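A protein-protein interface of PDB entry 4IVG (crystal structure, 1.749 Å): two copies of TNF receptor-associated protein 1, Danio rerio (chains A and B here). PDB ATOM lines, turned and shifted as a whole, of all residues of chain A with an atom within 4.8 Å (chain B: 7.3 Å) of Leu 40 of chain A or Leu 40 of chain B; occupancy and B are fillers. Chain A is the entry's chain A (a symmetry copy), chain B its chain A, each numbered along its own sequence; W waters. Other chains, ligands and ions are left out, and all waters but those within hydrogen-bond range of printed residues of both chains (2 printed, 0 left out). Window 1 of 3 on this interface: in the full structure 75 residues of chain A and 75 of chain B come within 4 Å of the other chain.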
ATOM      1  N   ALA A  35     -23.852  11.819  17.611  1.00  0.00           N
ATOM      2  CA  ALA A  35     -23.037  13.001  17.882  1.00  0.00           C
ATOM      3  C   ALA A  35     -21.761  12.633  18.637  1.00  0.00           C
ATOM      4  O   ALA A  35     -21.768  11.735  19.485  1.00  0.00           O
ATOM      5  CB  ALA A  35     -23.849  14.025  18.657  1.00  0.00           C
ATOM      6  N   GLU A  36     -20.663  13.309  18.314  1.00  0.00           N
ATOM      7  CA  GLU A  36     -19.403  13.086  19.011  1.00  0.00           C
ATOM      8  C   GLU A  36     -19.299  14.106  20.130  1.00  0.00           C
ATOM      9  O   GLU A  36     -18.908  15.255  19.907  1.00  0.00           O
ATOM     10  CB  GLU A  36     -18.220  13.230  18.057  1.00  0.00           C
ATOM     11  CG  GLU A  36     -16.899  12.730  18.624  1.00  0.00           C
ATOM     12  CD  GLU A  36     -15.882  12.431  17.536  1.00  0.00           C
ATOM     13  OE1 GLU A  36     -15.906  11.309  16.988  1.00  0.00           O
ATOM     14  OE2 GLU A  36     -15.064  13.320  17.218  1.00  0.00           O
ATOM     15  N   THR A  37     -19.660  13.677  21.338  1.00  0.00           N
ATOM     16  CA  THR A  37     -19.855  14.616  22.439  1.00  0.00           C
ATOM     17  C   THR A  37     -18.561  15.307  22.845  1.00  0.00           C
ATOM     18  O   THR A  37     -18.583  16.464  23.254  1.00  0.00           O
ATOM     19  CB  THR A  37     -20.526  13.951  23.660  1.00  0.00           C
ATOM     20  OG1 THR A  37     -19.663  12.940  24.177  1.00  0.00           O
ATOM     21  CG2 THR A  37     -21.862  13.316  23.264  1.00  0.00           C
ATOM     22  N   LYS A  38     -17.438  14.602  22.728  1.00  0.00           N
ATOM     23  CA  LYS A  38     -16.144  15.190  23.092  1.00  0.00           C
ATOM     24  C   LYS A  38     -15.785  16.359  22.199  1.00  0.00           C
ATOM     25  O   LYS A  38     -15.322  17.403  22.678  1.00  0.00           O
ATOM     26  CB  LYS A  38     -15.034  14.142  23.039  1.00  0.00           C
ATOM     27  CG  LYS A  38     -15.098  13.162  24.183  1.00  0.00           C
ATOM     28  CD  LYS A  38     -13.823  12.358  24.305  1.00  0.00           C
ATOM     29  CE  LYS A  38     -13.905  11.440  25.506  1.00  0.00           C
ATOM     30  NZ  LYS A  38     -13.153  10.180  25.279  1.00  0.00           N
ATOM     31  N   LYS A  39     -15.996  16.195  20.897  1.00  0.00           N
ATOM     32  CA  LYS A  39     -15.781  17.305  19.972  1.00  0.00           C
ATOM     33  C   LYS A  39     -16.726  18.451  20.273  1.00  0.00           C
ATOM     34  O   LYS A  39     -16.321  19.619  20.261  1.00  0.00           O
ATOM     35  CB  LYS A  39     -15.954  16.856  18.515  1.00  0.00           C
ATOM     36  CG  LYS A  39     -15.702  17.977  17.508  1.00  0.00           C
ATOM     37  CD  LYS A  39     -14.238  18.403  17.524  1.00  0.00           C
ATOM     38  CE  LYS A  39     -13.999  19.626  16.658  1.00  0.00           C
ATOM     39  NZ  LYS A  39     -12.560  19.782  16.296  1.00  0.00           N
ATOM     40  N   LEU A  40     -17.990  18.130  20.535  1.00  0.00           N
ATOM     41  CA  LEU A  40     -18.980  19.171  20.838  1.00  0.00           C
ATOM     42  C   LEU A  40     -18.590  19.978  22.060  1.00  0.00           C
ATOM     43  O   LEU A  40     -18.717  21.202  22.081  1.00  0.00           O
ATOM     44  CB  LEU A  40     -20.355  18.558  21.059  1.00  0.00           C
ATOM     45  CG  LEU A  40     -21.090  18.121  19.800  1.00  0.00           C
ATOM     46  CD1 LEU A  40     -22.290  17.291  20.204  1.00  0.00           C
ATOM     47  CD2 LEU A  40     -21.521  19.345  18.968  1.00  0.00           C
ATOM     48  N   LEU A  41     -18.142  19.286  23.102  1.00  0.00           N
ATOM     49  CA  LEU A  41     -17.641  20.001  24.276  1.00  0.00           C
ATOM     50  C   LEU A  41     -16.508  20.949  23.918  1.00  0.00           C
ATOM     51  O   LEU A  41     -16.470  22.073  24.394  1.00  0.00           O
ATOM     52  CB  LEU A  41     -17.188  19.008  25.343  1.00  0.00           C
ATOM     53  CG  LEU A  41     -18.372  18.275  25.955  1.00  0.00           C
ATOM     54  CD1 LEU A  41     -17.884  17.149  26.853  1.00  0.00           C
ATOM     55  CD2 LEU A  41     -19.247  19.268  26.731  1.00  0.00           C
ATOM     56  N   ASP A  42     -15.591  20.490  23.073  1.00  0.00           N
ATOM     57  CA  ASP A  42     -14.464  21.312  22.641  1.00  0.00           C
ATOM     58  C   ASP A  42     -14.935  22.531  21.846  1.00  0.00           C
ATOM     59  O   ASP A  42     -14.464  23.653  22.050  1.00  0.00           O
ATOM     60  CB  ASP A  42     -13.510  20.470  21.790  1.00  0.00           C
ATOM     61  CG  ASP A  42     -12.286  21.244  21.325  1.00  0.00           C
ATOM     62  OD1 ASP A  42     -11.354  21.439  22.142  1.00  0.00           O
ATOM     63  OD2 ASP A  42     -12.246  21.648  20.141  1.00  0.00           O
ATOM     64  N   ILE A  43     -15.875  22.305  20.934  1.00  0.00           N
ATOM     65  CA  ILE A  43     -16.447  23.382  20.125  1.00  0.00           C
ATOM     66  C   ILE A  43     -17.080  24.455  20.996  1.00  0.00           C
ATOM     67  O   ILE A  43     -16.875  25.655  20.794  1.00  0.00           O
ATOM     68  CB  ILE A  43     -17.506  22.818  19.135  1.00  0.00           C
ATOM     69  CG1 ILE A  43     -16.811  22.019  18.030  1.00  0.00           C
ATOM     70  CG2 ILE A  43     -18.389  23.951  18.591  1.00  0.00           C
ATOM     71  CD1 ILE A  43     -17.770  21.290  17.053  1.00  0.00           C
ATOM     72  N   VAL A  44     -17.836  24.017  21.994  1.00  0.00           N
ATOM     73  CA  VAL A  44     -18.505  24.956  22.885  1.00  0.00           C
ATOM     74  C   VAL A  44     -17.484  25.691  23.780  1.00  0.00           C
ATOM     75  O   VAL A  44     -17.653  26.867  24.118  1.00  0.00           O
ATOM     76  CB  VAL A  44     -19.585  24.205  23.696  1.00  0.00           C
ATOM     77  CG1 VAL A  44     -20.133  25.046  24.794  1.00  0.00           C
ATOM     78  CG2 VAL A  44     -20.733  23.764  22.769  1.00  0.00           C
ATOM     79  N   ILE A 118     -25.944  17.493  26.119  1.00  0.00           N
ATOM     80  CA  ILE A 118     -25.760  18.731  25.372  1.00  0.00           C
ATOM     81  C   ILE A 118     -26.929  18.900  24.421  1.00  0.00           C
ATOM     82  O   ILE A 118     -27.365  17.926  23.798  1.00  0.00           O
ATOM     83  CB  ILE A 118     -24.467  18.673  24.558  1.00  0.00           C
ATOM     84  CG1 ILE A 118     -23.270  18.515  25.497  1.00  0.00           C
ATOM     85  CG2 ILE A 118     -24.338  19.902  23.650  1.00  0.00           C
ATOM     86  CD1 ILE A 118     -22.043  17.938  24.843  1.00  0.00           C
ATOM     87  N   ALA A 119     -27.419  20.134  24.309  1.00  0.00           N
ATOM     88  CA  ALA A 119     -28.569  20.475  23.462  1.00  0.00           C
ATOM     89  C   ALA A 119     -29.872  19.977  24.058  1.00  0.00           C
ATOM     90  O   ALA A 119     -30.920  20.051  23.433  1.00  0.00           O
ATOM     91  CB  ALA A 119     -28.389  19.976  22.017  1.00  0.00           C
ATOM     92  N   GLN B  34     -23.749  13.075  26.937  1.00  0.00           N
ATOM     93  CA  GLN B  34     -24.491  12.648  25.760  1.00  0.00           C
ATOM     94  C   GLN B  34     -24.958  13.881  25.013  1.00  0.00           C
ATOM     95  O   GLN B  34     -24.698  15.003  25.437  1.00  0.00           O
ATOM     96  CB  GLN B  34     -25.696  11.805  26.158  1.00  0.00           C
ATOM     97  CG  GLN B  34     -25.336  10.436  26.711  1.00  0.00           C
ATOM     98  CD  GLN B  34     -26.540   9.701  27.264  1.00  0.00           C
ATOM     99  OE1 GLN B  34     -27.528  10.317  27.667  1.00  0.00           O
ATOM    100  NE2 GLN B  34     -26.463   8.374  27.290  1.00  0.00           N
ATOM    101  N   ALA B  35     -25.668  13.664  23.913  1.00  0.00           N
ATOM    102  CA  ALA B  35     -26.123  14.771  23.075  1.00  0.00           C
ATOM    103  C   ALA B  35     -27.501  14.486  22.483  1.00  0.00           C
ATOM    104  O   ALA B  35     -27.815  13.341  22.140  1.00  0.00           O
ATOM    105  CB  ALA B  35     -25.107  15.045  21.979  1.00  0.00           C
ATOM    106  N   GLU B  36     -28.332  15.520  22.382  1.00  0.00           N
ATOM    107  CA  GLU B  36     -29.648  15.379  21.775  1.00  0.00           C
ATOM    108  C   GLU B  36     -29.532  15.757  20.310  1.00  0.00           C
ATOM    109  O   GLU B  36     -29.557  16.939  19.956  1.00  0.00           O
ATOM    110  CB  GLU B  36     -30.668  16.277  22.471  1.00  0.00           C
ATOM    111  CG  GLU B  36     -32.114  15.979  22.101  1.00  0.00           C
ATOM    112  CD  GLU B  36     -33.093  16.518  23.130  1.00  0.00           C
ATOM    113  OE1 GLU B  36     -33.356  15.817  24.130  1.00  0.00           O
ATOM    114  OE2 GLU B  36     -33.594  17.648  22.948  1.00  0.00           O
ATOM    115  N   THR B  37     -29.399  14.741  19.459  1.00  0.00           N
ATOM    116  CA  THR B  37     -29.020  14.973  18.068  1.00  0.00           C
ATOM    117  C   THR B  37     -30.084  15.744  17.301  1.00  0.00           C
ATOM    118  O   THR B  37     -29.758  16.525  16.412  1.00  0.00           O
ATOM    119  CB  THR B  37     -28.659  13.663  17.337  1.00  0.00           C
ATOM    120  OG1 THR B  37     -29.812  12.825  17.277  1.00  0.00           O
ATOM    121  CG2 THR B  37     -27.539  12.922  18.074  1.00  0.00           C
ATOM    122  N   LYS B  38     -31.352  15.528  17.646  1.00  0.00           N
ATOM    123  CA  LYS B  38     -32.443  16.231  16.962  1.00  0.00           C
ATOM    124  C   LYS B  38     -32.384  17.726  17.196  1.00  0.00           C
ATOM    125  O   LYS B  38     -32.558  18.521  16.262  1.00  0.00           O
ATOM    126  CB  LYS B  38     -33.802  15.694  17.408  1.00  0.00           C
ATOM    127  CG  LYS B  38     -34.106  14.329  16.844  1.00  0.00           C
ATOM    128  CD  LYS B  38     -35.565  13.965  17.010  1.00  0.00           C
ATOM    129  CE  LYS B  38     -35.838  12.621  16.370  1.00  0.00           C
ATOM    130  NZ  LYS B  38     -36.904  11.881  17.092  1.00  0.00           N
ATOM    131  N   LYS B  39     -32.137  18.121  18.441  1.00  0.00           N
ATOM    132  CA  LYS B  39     -31.955  19.539  18.740  1.00  0.00           C
ATOM    133  C   LYS B  39     -30.743  20.093  18.017  1.00  0.00           C
ATOM    134  O   LYS B  39     -30.791  21.199  17.467  1.00  0.00           O
ATOM    135  CB  LYS B  39     -31.815  19.776  20.249  1.00  0.00           C
ATOM    136  CG  LYS B  39     -31.660  21.251  20.613  1.00  0.00           C
ATOM    137  CD  LYS B  39     -32.935  22.025  20.300  1.00  0.00           C
ATOM    138  CE  LYS B  39     -32.748  23.518  20.494  1.00  0.00           C
ATOM    139  NZ  LYS B  39     -34.050  24.231  20.640  1.00  0.00           N
ATOM    140  N   LEU B  40     -29.648  19.338  18.022  1.00  0.00           N
ATOM    141  CA  LEU B  40     -28.424  19.791  17.350  1.00  0.00           C
ATOM    142  C   LEU B  40     -28.650  20.025  15.870  1.00  0.00           C
ATOM    143  O   LEU B  40     -28.176  21.009  15.302  1.00  0.00           O
ATOM    144  CB  LEU B  40     -27.304  18.776  17.531  1.00  0.00           C
ATOM    145  CG  LEU B  40     -26.639  18.770  18.900  1.00  0.00           C
ATOM    146  CD1 LEU B  40     -25.763  17.539  19.006  1.00  0.00           C
ATOM    147  CD2 LEU B  40     -25.813  20.054  19.111  1.00  0.00           C
ATOM    148  N   LEU B  41     -29.353  19.097  15.229  1.00  0.00           N
ATOM    149  CA  LEU B  41     -29.708  19.308  13.825  1.00  0.00           C
ATOM    150  C   LEU B  41     -30.490  20.597  13.630  1.00  0.00           C
ATOM    151  O   LEU B  41     -30.235  21.337  12.692  1.00  0.00           O
ATOM    152  CB  LEU B  41     -30.503  18.117  13.299  1.00  0.00           C
ATOM    153  CG  LEU B  41     -29.629  16.878  13.175  1.00  0.00           C
ATOM    154  CD1 LEU B  41     -30.485  15.662  12.857  1.00  0.00           C
ATOM    155  CD2 LEU B  41     -28.563  17.107  12.096  1.00  0.00           C
ATOM    156  N   ASP B  42     -31.437  20.861  14.523  1.00  0.00           N
ATOM    157  CA  ASP B  42     -32.245  22.076  14.450  1.00  0.00           C
ATOM    158  C   ASP B  42     -31.385  23.328  14.634  1.00  0.00           C
ATOM    159  O   ASP B  42     -31.526  24.316  13.908  1.00  0.00           O
ATOM    160  CB  ASP B  42     -33.338  22.031  15.521  1.00  0.00           C
ATOM    161  CG  ASP B  42     -34.249  23.249  15.493  1.00  0.00           C
ATOM    162  OD1 ASP B  42     -35.141  23.309  14.613  1.00  0.00           O
ATOM    163  OD2 ASP B  42     -34.086  24.139  16.356  1.00  0.00           O
ATOM    164  N   ILE B  43     -30.488  23.282  15.613  1.00  0.00           N
ATOM    165  CA  ILE B  43     -29.573  24.391  15.881  1.00  0.00           C
ATOM    166  C   ILE B  43     -28.721  24.715  14.664  1.00  0.00           C
ATOM    167  O   ILE B  43     -28.556  25.876  14.282  1.00  0.00           O
ATOM    168  CB  ILE B  43     -28.654  24.062  17.092  1.00  0.00           C
ATOM    169  CG1 ILE B  43     -29.470  24.094  18.387  1.00  0.00           C
ATOM    170  CG2 ILE B  43     -27.445  25.009  17.122  1.00  0.00           C
ATOM    171  CD1 ILE B  43     -28.695  23.649  19.655  1.00  0.00           C
ATOM    172  N   VAL B  44     -28.197  23.673  14.033  1.00  0.00           N
ATOM    173  CA  VAL B  44     -27.351  23.863  12.862  1.00  0.00           C
ATOM    174  C   VAL B  44     -28.178  24.369  11.659  1.00  0.00           C
ATOM    175  O   VAL B  44     -27.700  25.156  10.836  1.00  0.00           O
ATOM    176  CB  VAL B  44     -26.596  22.549  12.562  1.00  0.00           C
ATOM    177  CG1 VAL B  44     -25.908  22.598  11.244  1.00  0.00           C
ATOM    178  CG2 VAL B  44     -25.561  22.269  13.668  1.00  0.00           C
ATOM    179  N   ALA B  45     -29.435  23.950  11.584  1.00  0.00           N
ATOM    180  CA  ALA B  45     -30.279  24.328  10.436  1.00  0.00           C
ATOM    181  C   ALA B  45     -30.801  25.764  10.565  1.00  0.00           C
ATOM    182  O   ALA B  45     -31.047  26.436   9.573  1.00  0.00           O
ATOM    183  CB  ALA B  45     -31.440  23.334  10.288  1.00  0.00           C
ATOM    184  N   ARG B  46     -30.942  26.241  11.796  1.00  0.00           N
ATOM    185  CA  ARG B  46     -31.657  27.492  12.052  1.00  0.00           C
ATOM    186  C   ARG B  46     -30.932  28.539  12.882  1.00  0.00           C
ATOM    187  O   ARG B  46     -31.288  29.716  12.835  1.00  0.00           O
ATOM    188  CB  ARG B  46     -32.967  27.180  12.772  1.00  0.00           C
ATOM    189  CG  ARG B  46     -33.886  26.230  12.032  1.00  0.00           C
ATOM    190  CD  ARG B  46     -35.121  25.947  12.869  1.00  0.00           C
ATOM    191  NE  ARG B  46     -35.578  27.152  13.553  1.00  0.00           N
ATOM    192  CZ  ARG B  46     -35.647  27.291  14.874  1.00  0.00           C
ATOM    193  NH1 ARG B  46     -35.305  26.290  15.673  1.00  0.00           N
ATOM    194  NH2 ARG B  46     -36.068  28.438  15.390  1.00  0.00           N
ATOM    195  N   ILE B 118     -22.639  13.956  13.928  1.00  0.00           N
ATOM    196  CA  ILE B 118     -22.403  15.392  14.013  1.00  0.00           C
ATOM    197  C   ILE B 118     -21.171  15.630  14.864  1.00  0.00           C
ATOM    198  O   ILE B 118     -20.991  14.968  15.891  1.00  0.00           O
ATOM    199  CB  ILE B 118     -23.596  16.088  14.670  1.00  0.00           C
ATOM    200  CG1 ILE B 118     -24.851  15.873  13.822  1.00  0.00           C
ATOM    201  CG2 ILE B 118     -23.299  17.574  14.905  1.00  0.00           C
ATOM    202  CD1 ILE B 118     -26.143  16.040  14.578  1.00  0.00           C
ATOM    203  N   ALA B 119     -20.338  16.578  14.436  1.00  0.00           N
ATOM    204  CA  ALA B 119     -19.080  16.919  15.114  1.00  0.00           C
ATOM    205  C   ALA B 119     -18.024  15.851  14.905  1.00  0.00           C
ATOM    206  O   ALA B 119     -16.957  15.896  15.501  1.00  0.00           O
ATOM    207  CB  ALA B 119     -19.293  17.209  16.610  1.00  0.00           C
ATOM    208  N   ARG B 120     -18.295  14.885  14.039  1.00  0.00           N
ATOM    209  CA  ARG B 120     -17.242  13.939  13.707  1.00  0.00           C
ATOM    210  C   ARG B 120     -16.652  14.279  12.349  1.00  0.00           C
ATOM    211  O   ARG B 120     -17.378  14.420  11.360  1.00  0.00           O
ATOM    212  CB  ARG B 120     -17.742  12.501  13.700  1.00  0.00           C
ATOM    213  CG  ARG B 120     -16.625  11.538  13.352  1.00  0.00           C
ATOM    214  CD  ARG B 120     -17.126  10.132  13.228  1.00  0.00           C
ATOM    215  NE  ARG B 120     -17.674   9.683  14.495  1.00  0.00           N
ATOM    216  CZ  ARG B 120     -16.973   9.049  15.422  1.00  0.00           C
ATOM    217  NH1 ARG B 120     -15.694   8.772  15.211  1.00  0.00           N
ATOM    218  NH2 ARG B 120     -17.556   8.684  16.554  1.00  0.00           N
ATOM    219  N   PHE B 144     -14.582  21.091  12.068  1.00  0.00           N
ATOM    220  CA  PHE B 144     -15.632  20.990  13.088  1.00  0.00           C
ATOM    221  C   PHE B 144     -16.473  19.717  13.015  1.00  0.00           C
ATOM    222  O   PHE B 144     -16.941  19.234  14.035  1.00  0.00           O
ATOM    223  CB  PHE B 144     -16.572  22.201  13.026  1.00  0.00           C
ATOM    224  CG  PHE B 144     -15.899  23.506  13.308  1.00  0.00           C
ATOM    225  CD1 PHE B 144     -15.294  23.725  14.537  1.00  0.00           C
ATOM    226  CD2 PHE B 144     -15.874  24.523  12.357  1.00  0.00           C
ATOM    227  CE1 PHE B 144     -14.660  24.940  14.823  1.00  0.00           C
ATOM    228  CE2 PHE B 144     -15.239  25.744  12.643  1.00  0.00           C
ATOM    229  CZ  PHE B 144     -14.633  25.945  13.874  1.00  0.00           C
ATOM    230  N   VAL B 146     -19.407  19.592  11.129  1.00  0.00           N
ATOM    231  CA  VAL B 146     -20.807  20.032  11.017  1.00  0.00           C
ATOM    232  C   VAL B 146     -21.211  20.580   9.655  1.00  0.00           C
ATOM    233  O   VAL B 146     -22.403  20.704   9.377  1.00  0.00           O
ATOM    234  CB  VAL B 146     -21.201  21.106  12.066  1.00  0.00           C
ATOM    235  CG1 VAL B 146     -20.879  20.627  13.493  1.00  0.00           C
ATOM    236  CG2 VAL B 146     -20.515  22.447  11.756  1.00  0.00           C
ATOM    237  N   TYR B 149     -24.203  19.380   7.331  1.00  0.00           N
ATOM    238  CA  TYR B 149     -25.596  19.560   7.767  1.00  0.00           C
ATOM    239  C   TYR B 149     -26.188  20.886   7.334  1.00  0.00           C
ATOM    240  O   TYR B 149     -27.405  21.059   7.369  1.00  0.00           O
ATOM    241  CB  TYR B 149     -25.725  19.375   9.283  1.00  0.00           C
ATOM    242  CG  TYR B 149     -25.158  18.054   9.702  1.00  0.00           C
ATOM    243  CD1 TYR B 149     -25.853  16.875   9.478  1.00  0.00           C
ATOM    244  CD2 TYR B 149     -23.907  17.981  10.277  1.00  0.00           C
ATOM    245  CE1 TYR B 149     -25.311  15.655   9.845  1.00  0.00           C
ATOM    246  CE2 TYR B 149     -23.360  16.790  10.648  1.00  0.00           C
ATOM    247  CZ  TYR B 149     -24.057  15.636  10.428  1.00  0.00           C
ATOM    248  OH  TYR B 149     -23.450  14.476  10.827  1.00  0.00           O
ATOM    249  N   LEU B 343     -17.899  28.405  15.056  1.00  0.00           N
ATOM    250  CA  LEU B 343     -18.528  27.238  14.431  1.00  0.00           C
ATOM    251  C   LEU B 343     -19.202  27.596  13.104  1.00  0.00           C
ATOM    252  O   LEU B 343     -19.314  26.764  12.195  1.00  0.00           O
ATOM    253  CB  LEU B 343     -19.539  26.642  15.398  1.00  0.00           C
ATOM    254  CG  LEU B 343     -20.179  25.337  14.956  1.00  0.00           C
ATOM    255  CD1 LEU B 343     -19.111  24.276  14.712  1.00  0.00           C
ATOM    256  CD2 LEU B 343     -21.192  24.892  15.991  1.00  0.00           C
HETATM  257  O   HOH W   1     -34.171  20.174  24.400  1.00  0.00           O
HETATM  258  O   HOH W   2     -13.887  14.618  14.820  1.00  0.00           O
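The backbone NH (N) of Ile 118 of chain A sits at hydrogen-bond distance from the backbone carbonyl oxygen (O) of Gln 34 of chain B (2.9 Å).
The backbone carbonyl oxygen (O) of Ile 118 of chain A sits at hydrogen-bond distance from the backbone NH (N) of Glu 36 of chain B.
N of Glu 36 of chain A is in hydrogen-bond range of O of Ile 118 of chain B (3.0 Å).
NH1 of Arg 120 of chain B lies within salt-bridge range of OE1 of Glu 36 of chain A (3.1 Å).
N of Ile 118 of chain B sits at hydrogen-bond distance from OH of Tyr 149 of chain B (3.2 Å).
Among the printed residues, pairs that only touch across the chains: Ala 35 of chain A with Ala 35 of chain B (3.7 Å), Ala 35 of chain A with Thr 37 of chain B (3.9 Å), Ala 35 of chain A with Ile 118 of chain B (3.5 Å), Glu 36 of chain A with Ala 119 of chain B (3.6 Å), Thr 37 of chain A with Gln 34 of chain B (3.6 Å), Thr 37 of chain A with Ala 35 of chain B (3.9 Å), Lys 39 of chain A with Ala 119 of chain B (3.2 Å), Lys 39 of chain A with Phe 144 of chain B (3.9 Å), Leu 40 of chain A with Leu 40 of chain B (3.7 Å), Leu 40 of chain A with Ala 119 of chain B (3.8 Å), Ile 43 of chain A with Phe 144 of chain B (3.7 Å), Ile 43 of chain A with Leu 343 of chain B (3.9 Å), Ile 118 of chain A with Ala 35 of chain B (3.5 Å), Ala 119 of chain A with Glu 36 of chain B (3.6 Å), Ala 119 of chain A with Lys 39 of chain B (3.2 Å) and Ala 119 of chain A with Leu 40 of chain B (3.8 Å).
Printed residues of chain B within 4 Å of Leu 40 of chain A: Leu 40 and Ala 119.
Of the printed residues of chain A, Leu 40 of chain B touches Leu 40 and Ala 119.
Printed residues of chain A within 4 Å of Ala 119 of chain B: Glu 36 (3.6 Å), Lys 39 (3.2 Å) and Leu 40 (3.8 Å).
Of the printed residues of chain A, Lys 39 of chain B touches Ala 119.
Printed residues of chain A within 4 Å of Leu 343 of chain B: Ile 43.
Of the printed residues of chain A, Ile 118 of chain B touches Ala 35 (3.5 Å) and Glu 36 (3.0 Å).
Printed residues of chain B within 4 Å of Ile 118 of chain A: Gln 34, Ala 35 and Glu 36.
Val 146 of chain B touches none of the printed residues of chain A.
The nearest printed residue of chain B that does not touch Leu 40 of chain A is Ala 35 of chain B (4.02 Å).
The nearest printed residue of chain A that does not touch Leu 40 of chain B is Ala 35 of chain A (4.02 Å).
Ala 35 of chain B touches its own counterpart, Ala 35 of chain A.
Ala 35 of chain A touches Thr 37 of chain B, and with the chains exchanged Thr 37 of chain A touches Ala 35 of chain B.
Glu 36 of chain A touches Ala 119 of chain B, and with the chains exchanged Ala 119 of chain A touches Glu 36 of chain B.
Lys 39 of chain A touches Ala 119 of chain B, and with the chains exchanged Ala 119 of chain A touches Lys 39 of chain B.
12 positions are printed for both chains.
Water W1 lies within hydrogen-bond range of OE2 of Glu 36 of chain B and O of Ala 119 of chain A.
Water W2 lies within hydrogen-bond range of OE2 of Glu 36 of chain A and O of Ala 119 of chain B.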
